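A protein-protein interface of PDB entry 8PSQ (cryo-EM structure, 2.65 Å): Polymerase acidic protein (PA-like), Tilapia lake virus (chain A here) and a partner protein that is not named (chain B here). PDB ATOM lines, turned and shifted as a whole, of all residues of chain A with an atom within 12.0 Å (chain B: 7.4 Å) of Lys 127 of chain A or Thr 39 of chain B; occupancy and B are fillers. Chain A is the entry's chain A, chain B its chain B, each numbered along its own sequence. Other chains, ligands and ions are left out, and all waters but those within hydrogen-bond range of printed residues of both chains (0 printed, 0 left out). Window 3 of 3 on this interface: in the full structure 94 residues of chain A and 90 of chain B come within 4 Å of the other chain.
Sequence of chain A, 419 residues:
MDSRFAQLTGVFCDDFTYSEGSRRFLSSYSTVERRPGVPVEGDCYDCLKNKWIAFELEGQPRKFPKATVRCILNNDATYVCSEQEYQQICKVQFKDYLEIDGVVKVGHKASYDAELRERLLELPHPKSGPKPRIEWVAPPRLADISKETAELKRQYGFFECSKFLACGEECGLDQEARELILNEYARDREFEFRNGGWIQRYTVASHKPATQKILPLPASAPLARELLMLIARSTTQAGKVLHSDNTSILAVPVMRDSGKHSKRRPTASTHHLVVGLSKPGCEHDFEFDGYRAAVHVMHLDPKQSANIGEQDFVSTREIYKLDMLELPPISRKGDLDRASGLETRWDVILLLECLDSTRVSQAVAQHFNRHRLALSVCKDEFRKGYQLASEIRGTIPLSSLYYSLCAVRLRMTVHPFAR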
ATOM      1  N   LEU A 121      -9.882  -1.458  -7.257  1.00  0.00           N
ATOM      2  CA  LEU A 121      -9.235  -2.737  -6.989  1.00  0.00           C
ATOM      3  C   LEU A 121      -7.719  -2.592  -6.966  1.00  0.00           C
ATOM      4  O   LEU A 121      -7.046  -3.178  -6.111  1.00  0.00           O
ATOM      5  CB  LEU A 121      -9.652  -3.766  -8.040  1.00  0.00           C
ATOM      6  CG  LEU A 121     -10.733  -4.782  -7.664  1.00  0.00           C
ATOM      7  CD1 LEU A 121     -10.909  -5.779  -8.792  1.00  0.00           C
ATOM      8  CD2 LEU A 121     -10.401  -5.509  -6.369  1.00  0.00           C
ATOM      9  N   GLU A 122      -7.162  -1.819  -7.899  1.00  0.00           N
ATOM     10  CA  GLU A 122      -5.713  -1.668  -7.958  1.00  0.00           C
ATOM     11  C   GLU A 122      -5.154  -0.812  -6.830  1.00  0.00           C
ATOM     12  O   GLU A 122      -3.933  -0.787  -6.647  1.00  0.00           O
ATOM     13  CB  GLU A 122      -5.299  -1.066  -9.303  1.00  0.00           C
ATOM     14  CG  GLU A 122      -5.663  -1.907 -10.521  1.00  0.00           C
ATOM     15  CD  GLU A 122      -5.408  -3.391 -10.322  1.00  0.00           C
ATOM     16  OE1 GLU A 122      -4.349  -3.747  -9.763  1.00  0.00           O
ATOM     17  OE2 GLU A 122      -6.266  -4.203 -10.728  1.00  0.00           O
ATOM     18  N   LEU A 123      -5.997  -0.121  -6.076  1.00  0.00           N
ATOM     19  CA  LEU A 123      -5.530   0.749  -5.007  1.00  0.00           C
ATOM     20  C   LEU A 123      -5.306  -0.042  -3.726  1.00  0.00           C
ATOM     21  O   LEU A 123      -5.759  -1.183  -3.598  1.00  0.00           O
ATOM     22  CB  LEU A 123      -6.538   1.870  -4.770  1.00  0.00           C
ATOM     23  CG  LEU A 123      -6.475   3.013  -5.787  1.00  0.00           C
ATOM     24  CD1 LEU A 123      -7.715   3.883  -5.701  1.00  0.00           C
ATOM     25  CD2 LEU A 123      -5.223   3.849  -5.594  1.00  0.00           C
ATOM     26  N   PRO A 124      -4.593   0.532  -2.755  1.00  0.00           N
ATOM     27  CA  PRO A 124      -4.303  -0.207  -1.519  1.00  0.00           C
ATOM     28  C   PRO A 124      -5.566  -0.548  -0.742  1.00  0.00           C
ATOM     29  O   PRO A 124      -6.576   0.156  -0.810  1.00  0.00           O
ATOM     30  CB  PRO A 124      -3.407   0.754  -0.729  1.00  0.00           C
ATOM     31  CG  PRO A 124      -2.915   1.746  -1.719  1.00  0.00           C
ATOM     32  CD  PRO A 124      -3.976   1.867  -2.753  1.00  0.00           C
ATOM     33  N   HIS A 125      -5.498  -1.648   0.003  1.00  0.00           N
ATOM     34  CA  HIS A 125      -6.588  -2.122   0.838  1.00  0.00           C
ATOM     35  C   HIS A 125      -6.086  -2.352   2.255  1.00  0.00           C
ATOM     36  O   HIS A 125      -4.897  -2.612   2.463  1.00  0.00           O
ATOM     37  CB  HIS A 125      -7.181  -3.430   0.297  1.00  0.00           C
ATOM     38  CG  HIS A 125      -7.787  -3.304  -1.065  1.00  0.00           C
ATOM     39  ND1 HIS A 125      -9.127  -3.050  -1.263  1.00  0.00           N
ATOM     40  CD2 HIS A 125      -7.238  -3.399  -2.299  1.00  0.00           C
ATOM     41  CE1 HIS A 125      -9.377  -2.992  -2.558  1.00  0.00           C
ATOM     42  NE2 HIS A 125      -8.246  -3.201  -3.209  1.00  0.00           N
ATOM     43  N   PRO A 126      -6.965  -2.255   3.251  1.00  0.00           N
ATOM     44  CA  PRO A 126      -6.548  -2.525   4.629  1.00  0.00           C
ATOM     45  C   PRO A 126      -6.372  -4.013   4.889  1.00  0.00           C
ATOM     46  O   PRO A 126      -6.918  -4.870   4.191  1.00  0.00           O
ATOM     47  CB  PRO A 126      -7.692  -1.946   5.465  1.00  0.00           C
ATOM     48  CG  PRO A 126      -8.874  -2.032   4.582  1.00  0.00           C
ATOM     49  CD  PRO A 126      -8.379  -1.849   3.175  1.00  0.00           C
ATOM     50  N   LYS A 127      -5.596  -4.310   5.927  1.00  0.00           N
ATOM     51  CA  LYS A 127      -5.347  -5.677   6.361  1.00  0.00           C
ATOM     52  C   LYS A 127      -6.116  -5.959   7.644  1.00  0.00           C
ATOM     53  O   LYS A 127      -6.319  -5.062   8.468  1.00  0.00           O
ATOM     54  CB  LYS A 127      -3.854  -5.915   6.588  1.00  0.00           C
ATOM     55  CG  LYS A 127      -2.998  -5.708   5.353  1.00  0.00           C
ATOM     56  CD  LYS A 127      -1.516  -5.744   5.698  1.00  0.00           C
ATOM     57  CE  LYS A 127      -0.636  -5.258   4.552  1.00  0.00           C
ATOM     58  NZ  LYS A 127      -1.387  -4.964   3.301  1.00  0.00           N
ATOM     59  N   SER A 128      -6.541  -7.209   7.809  1.00  0.00           N
ATOM     60  CA  SER A 128      -7.290  -7.590   8.999  1.00  0.00           C
ATOM     61  C   SER A 128      -6.476  -7.294  10.252  1.00  0.00           C
ATOM     62  O   SER A 128      -5.294  -7.637  10.336  1.00  0.00           O
ATOM     63  CB  SER A 128      -7.651  -9.073   8.940  1.00  0.00           C
ATOM     64  OG  SER A 128      -8.941  -9.264   8.389  1.00  0.00           O
ATOM     65  N   GLY A 129      -7.116  -6.655  11.227  1.00  0.00           N
ATOM     66  CA  GLY A 129      -6.457  -6.291  12.457  1.00  0.00           C
ATOM     67  C   GLY A 129      -6.460  -7.420  13.465  1.00  0.00           C
ATOM     68  O   GLY A 129      -7.067  -8.474  13.252  1.00  0.00           O
ATOM     69  N   PRO A 130      -5.778  -7.219  14.590  1.00  0.00           N
ATOM     70  CA  PRO A 130      -5.741  -8.259  15.623  1.00  0.00           C
ATOM     71  C   PRO A 130      -6.970  -8.207  16.515  1.00  0.00           C
ATOM     72  O   PRO A 130      -7.444  -7.134  16.896  1.00  0.00           O
ATOM     73  CB  PRO A 130      -4.468  -7.926  16.409  1.00  0.00           C
ATOM     74  CG  PRO A 130      -4.293  -6.446  16.240  1.00  0.00           C
ATOM     75  CD  PRO A 130      -5.012  -6.024  14.979  1.00  0.00           C
ATOM     76  N   LYS A 131      -7.481  -9.383  16.852  1.00  0.00           N
ATOM     77  CA  LYS A 131      -8.662  -9.476  17.698  1.00  0.00           C
ATOM     78  C   LYS A 131      -8.295  -9.112  19.133  1.00  0.00           C
ATOM     79  O   LYS A 131      -7.418  -9.757  19.715  1.00  0.00           O
ATOM     80  CB  LYS A 131      -9.241 -10.881  17.648  1.00  0.00           C
ATOM     81  CG  LYS A 131     -10.626 -10.995  18.253  1.00  0.00           C
ATOM     82  CD  LYS A 131     -11.688 -11.222  17.193  1.00  0.00           C
ATOM     83  CE  LYS A 131     -12.927 -11.872  17.781  1.00  0.00           C
ATOM     84  NZ  LYS A 131     -13.314 -11.270  19.088  1.00  0.00           N
ATOM     85  N   PRO A 132      -8.923  -8.103  19.732  1.00  0.00           N
ATOM     86  CA  PRO A 132      -8.570  -7.742  21.109  1.00  0.00           C
ATOM     87  C   PRO A 132      -9.043  -8.784  22.107  1.00  0.00           C
ATOM     88  O   PRO A 132     -10.031  -9.490  21.888  1.00  0.00           O
ATOM     89  CB  PRO A 132      -9.289  -6.405  21.320  1.00  0.00           C
ATOM     90  CG  PRO A 132     -10.452  -6.461  20.401  1.00  0.00           C
ATOM     91  CD  PRO A 132     -10.018  -7.266  19.209  1.00  0.00           C
ATOM     92  N   ARG B  33      -3.216   7.725  12.681  1.00  0.00           N
ATOM     93  CA  ARG B  33      -4.025   6.626  13.196  1.00  0.00           C
ATOM     94  C   ARG B  33      -4.673   5.845  12.060  1.00  0.00           C
ATOM     95  O   ARG B  33      -4.698   4.608  12.080  1.00  0.00           O
ATOM     96  CB  ARG B  33      -5.093   7.156  14.152  1.00  0.00           C
ATOM     97  CG  ARG B  33      -4.560   7.702  15.466  1.00  0.00           C
ATOM     98  CD  ARG B  33      -3.850   6.614  16.285  1.00  0.00           C
ATOM     99  NE  ARG B  33      -2.407   6.517  16.079  1.00  0.00           N
ATOM    100  CZ  ARG B  33      -1.556   7.536  16.029  1.00  0.00           C
ATOM    101  NH1 ARG B  33      -1.916   8.765  16.363  1.00  0.00           N
ATOM    102  NH2 ARG B  33      -0.293   7.308  15.680  1.00  0.00           N
ATOM    103  N   ALA B  34      -5.207   6.552  11.062  1.00  0.00           N
ATOM    104  CA  ALA B  34      -5.821   5.870   9.927  1.00  0.00           C
ATOM    105  C   ALA B  34      -4.802   5.019   9.179  1.00  0.00           C
ATOM    106  O   ALA B  34      -5.097   3.887   8.783  1.00  0.00           O
ATOM    107  CB  ALA B  34      -6.464   6.886   8.986  1.00  0.00           C
ATOM    108  N   SER B  35      -3.594   5.550   8.975  1.00  0.00           N
ATOM    109  CA  SER B  35      -2.557   4.783   8.292  1.00  0.00           C
ATOM    110  C   SER B  35      -2.175   3.540   9.086  1.00  0.00           C
ATOM    111  O   SER B  35      -2.016   2.453   8.517  1.00  0.00           O
ATOM    112  CB  SER B  35      -1.331   5.662   8.052  1.00  0.00           C
ATOM    113  OG  SER B  35      -1.671   6.815   7.305  1.00  0.00           O
ATOM    114  N   GLU B  36      -2.023   3.680  10.405  1.00  0.00           N
ATOM    115  CA  GLU B  36      -1.678   2.528  11.228  1.00  0.00           C
ATOM    116  C   GLU B  36      -2.770   1.470  11.172  1.00  0.00           C
ATOM    117  O   GLU B  36      -2.478   0.271  11.095  1.00  0.00           O
ATOM    118  CB  GLU B  36      -1.433   2.965  12.672  1.00  0.00           C
ATOM    119  CG  GLU B  36      -0.014   3.426  12.943  1.00  0.00           C
ATOM    120  CD  GLU B  36       0.040   4.641  13.849  1.00  0.00           C
ATOM    121  OE1 GLU B  36      -0.814   4.750  14.755  1.00  0.00           O
ATOM    122  OE2 GLU B  36       0.935   5.490  13.654  1.00  0.00           O
ATOM    123  N   ILE B  37      -4.034   1.891  11.215  1.00  0.00           N
ATOM    124  CA  ILE B  37      -5.128   0.928  11.123  1.00  0.00           C
ATOM    125  C   ILE B  37      -5.124   0.259   9.756  1.00  0.00           C
ATOM    126  O   ILE B  37      -5.434  -0.931   9.628  1.00  0.00           O
ATOM    127  CB  ILE B  37      -6.474   1.613  11.419  1.00  0.00           C
ATOM    128  CG1 ILE B  37      -6.563   1.972  12.902  1.00  0.00           C
ATOM    129  CG2 ILE B  37      -7.628   0.705  11.017  1.00  0.00           C
ATOM    130  CD1 ILE B  37      -7.638   2.974  13.228  1.00  0.00           C
ATOM    131  N   MET B  38      -4.773   1.011   8.713  1.00  0.00           N
ATOM    132  CA  MET B  38      -4.640   0.419   7.387  1.00  0.00           C
ATOM    133  C   MET B  38      -3.565  -0.659   7.377  1.00  0.00           C
ATOM    134  O   MET B  38      -3.732  -1.710   6.747  1.00  0.00           O
ATOM    135  CB  MET B  38      -4.319   1.505   6.361  1.00  0.00           C
ATOM    136  CG  MET B  38      -4.589   1.093   4.930  1.00  0.00           C
ATOM    137  SD  MET B  38      -6.194   1.638   4.328  1.00  0.00           S
ATOM    138  CE  MET B  38      -5.930   1.528   2.563  1.00  0.00           C
ATOM    139  N   THR B  39      -2.449  -0.414   8.066  1.00  0.00           N
ATOM    140  CA  THR B  39      -1.390  -1.416   8.138  1.00  0.00           C
ATOM    141  C   THR B  39      -1.896  -2.723   8.739  1.00  0.00           C
ATOM    142  O   THR B  39      -1.368  -3.795   8.426  1.00  0.00           O
ATOM    143  CB  THR B  39      -0.214  -0.866   8.951  1.00  0.00           C
ATOM    144  OG1 THR B  39       0.597  -0.032   8.116  1.00  0.00           O
ATOM    145  CG2 THR B  39       0.649  -1.988   9.514  1.00  0.00           C
ATOM    146  N   GLY B  40      -2.915  -2.660   9.591  1.00  0.00           N
ATOM    147  CA  GLY B  40      -3.477  -3.854  10.191  1.00  0.00           C
ATOM    148  C   GLY B  40      -2.802  -4.232  11.492  1.00  0.00           C
ATOM    149  O   GLY B  40      -2.655  -5.418  11.798  1.00  0.00           O
ATOM    150  N   LYS B  41      -2.389  -3.230  12.270  1.00  0.00           N
ATOM    151  CA  LYS B  41      -1.642  -3.457  13.496  1.00  0.00           C
ATOM    152  C   LYS B  41      -2.307  -2.904  14.748  1.00  0.00           C
ATOM    153  O   LYS B  41      -1.928  -3.309  15.852  1.00  0.00           O
ATOM    154  CB  LYS B  41      -0.235  -2.847  13.380  1.00  0.00           C
ATOM    155  CG  LYS B  41       0.885  -3.874  13.305  1.00  0.00           C
ATOM    156  CD  LYS B  41       0.726  -4.793  12.104  1.00  0.00           C
ATOM    157  CE  LYS B  41       2.068  -5.146  11.484  1.00  0.00           C
ATOM    158  NZ  LYS B  41       2.095  -6.544  10.976  1.00  0.00           N
ATOM    159  N   SER B  42      -3.280  -2.001  14.621  1.00  0.00           N
ATOM    160  CA  SER B  42      -3.910  -1.377  15.778  1.00  0.00           C
ATOM    161  C   SER B  42      -5.367  -1.793  15.939  1.00  0.00           C
ATOM    162  O   SER B  42      -5.754  -2.289  16.999  1.00  0.00           O
ATOM    163  CB  SER B  42      -3.798   0.150  15.671  1.00  0.00           C
ATOM    164  OG  SER B  42      -4.483   0.633  14.532  1.00  0.00           O
ATOM    165  N   TYR B  43      -6.188  -1.607  14.908  1.00  0.00           N
ATOM    166  CA  TYR B  43      -7.605  -1.927  14.972  1.00  0.00           C
ATOM    167  C   TYR B  43      -8.012  -2.592  13.666  1.00  0.00           C
ATOM    168  O   TYR B  43      -7.204  -2.747  12.745  1.00  0.00           O
ATOM    169  CB  TYR B  43      -8.442  -0.673  15.247  1.00  0.00           C
ATOM    170  CG  TYR B  43      -8.122  -0.006  16.563  1.00  0.00           C
ATOM    171  CD1 TYR B  43      -8.690  -0.455  17.745  1.00  0.00           C
ATOM    172  CD2 TYR B  43      -7.252   1.072  16.625  1.00  0.00           C
ATOM    173  CE1 TYR B  43      -8.402   0.148  18.949  1.00  0.00           C
ATOM    174  CE2 TYR B  43      -6.957   1.683  17.826  1.00  0.00           C
ATOM    175  CZ  TYR B  43      -7.536   1.216  18.985  1.00  0.00           C
ATOM    176  OH  TYR B  43      -7.247   1.819  20.186  1.00  0.00           O
ATOM    177  N   ASN B  44      -9.277  -2.988  13.585  1.00  0.00           N
ATOM    178  CA  ASN B  44      -9.786  -3.721  12.435  1.00  0.00           C
ATOM    179  C   ASN B  44     -10.569  -2.793  11.517  1.00  0.00           C
ATOM    180  O   ASN B  44     -11.508  -2.122  11.953  1.00  0.00           O
ATOM    181  CB  ASN B  44     -10.674  -4.878  12.886  1.00  0.00           C
ATOM    182  CG  ASN B  44     -11.069  -5.786  11.744  1.00  0.00           C
ATOM    183  OD1 ASN B  44     -10.231  -6.189  10.941  1.00  0.00           O
ATOM    184  ND2 ASN B  44     -12.351  -6.107  11.662  1.00  0.00           N
ATOM    185  N   ALA B  45     -10.183  -2.771  10.240  1.00  0.00           N
ATOM    186  CA  ALA B  45     -10.891  -2.012   9.218  1.00  0.00           C
ATOM    187  C   ALA B  45     -11.399  -2.899   8.088  1.00  0.00           C
ATOM    188  O   ALA B  45     -11.821  -2.377   7.050  1.00  0.00           O
ATOM    189  CB  ALA B  45      -9.992  -0.912   8.653  1.00  0.00           C
ATOM    190  N   VAL B  46     -11.374  -4.218   8.260  1.00  0.00           N
ATOM    191  CA  VAL B  46     -11.851  -5.159   7.252  1.00  0.00           C
ATOM    192  C   VAL B  46     -13.211  -5.682   7.686  1.00  0.00           C
ATOM    193  O   VAL B  46     -13.347  -6.266   8.768  1.00  0.00           O
ATOM    194  CB  VAL B  46     -10.856  -6.315   7.053  1.00  0.00           C
ATOM    195  CG1 VAL B  46     -11.422  -7.342   6.087  1.00  0.00           C
ATOM    196  CG2 VAL B  46      -9.522  -5.789   6.552  1.00  0.00           C
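N of Gly 129 of chain A lies within hydrogen-bond range of OD1 of Asn 44 of chain B (3.2 Å). The backbone NH (N) of Lys 127 of chain A is in hydrogen-bond range of the backbone carbonyl oxygen (O) of Met 38 of chain B (3.3 Å).
The backbone carbonyl oxygen (O) of Val 46 of chain B is in hydrogen-bond range of the side-chain amide nitrogen (ND2) of Asn 44 of chain B (3.1 Å). A ring nitrogen (NE2) of His 125 of chain A sits at hydrogen-bond distance from the backbone carbonyl oxygen of Leu 121 of chain A (3.1 Å). The backbone carbonyl oxygen (O) of Leu 123 of chain A lies close to a ring nitrogen (NE2) of His 125 of chain A (3.2 Å).
Met 38 of chain B touches Pro 124 of chain A (CE to O, 3.7 Å). Pro 126 of chain A touches Met 38 of chain B. Pro 126 of chain A touches Ala 45 of chain B. O of Pro 126 of chain A touches CG2 of Val 46 of chain B (3.6 Å). Lys 127 of chain A touches Thr 39 of chain B (CD to O, 3.4 Å). Ser 128 of chain A touches Asn 44 of chain B. N of Ser 128 of chain A touches CG2 of Val 46 of chain B, 3.5 Å away. Gly 40 of chain B touches Gly 129 of chain A (O to CA, 3.96 Å). Gly 129 of chain A touches Tyr 43 of chain B (CA to O, 3.6 Å). CG of Pro 130 of chain A touches O of Lys 41 of chain B, at 3.9 Å.
Lys 127 of chain A touches just these residues of chain B: Met 38 (3.3 Å), Thr 39 (3.4 Å), Gly 40 (3.5 Å) and Val 46 (3.6 Å). Of chain A, only Lys 127 (3.4 Å) comes within 4 Å of Thr 39 of chain B. No residue of chain A comes within 4 Å of Ser 35 of chain B. Met 38 of chain B touches four residues of chain A. Printed residues of chain A within 4 Å of Lys 41 of chain B: Pro 130. Of chain A, only Ser 128 (3.8 Å) and Gly 129 (3.2 Å) come within 4 Å of Asn 44 of chain B. Val 46 of chain B touches just these residues of chain A: Pro 126 (3.6 Å), Lys 127 (3.6 Å) and Ser 128 (3.5 Å). Printed residues of chain B within 4 Å of Pro 124 of chain A: Met 38 (3.7 Å). Of the printed residues of chain A, Tyr 43 of chain B touches Gly 129. Of the printed residues of chain B, Pro 126 of chain A touches Met 38 (3.6 Å), Ala 45 (3.9 Å) and Val 46 (3.6 Å). Printed residues of chain B within 4 Å of Ser 128 of chain A: Gly 40 (3.7 Å), Asn 44 (3.8 Å) and Val 46 (3.5 Å). The nearest residue of chain B that does not touch Lys 127 of chain A is Ile 37 of chain B (4.4 Å). The nearest residue of chain A that does not touch Thr 39 of chain B is Pro 126 of chain A (5.8 Å). The nearest printed residue of chain B that does not touch Ser 128 of chain A is Tyr 43 of chain B (5.2 Å).
Hydrophobic or aromatic side chains of chain B within 4 Å of the printed part of chain A: Met 38 and Val 46. Of the 12 printed residues of chain A, 7 touch a printed residue of chain B. Hydrophobic or aromatic side chains of chain A that line the printed part of chain B: Pro 126 and Pro 130. Among the printed residues, 16 pairs touch across the chains. Among the printed residues, no Asp or Glu carboxylate lies within 4 Å of a Lys or Arg side-chain nitrogen of the other chain.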
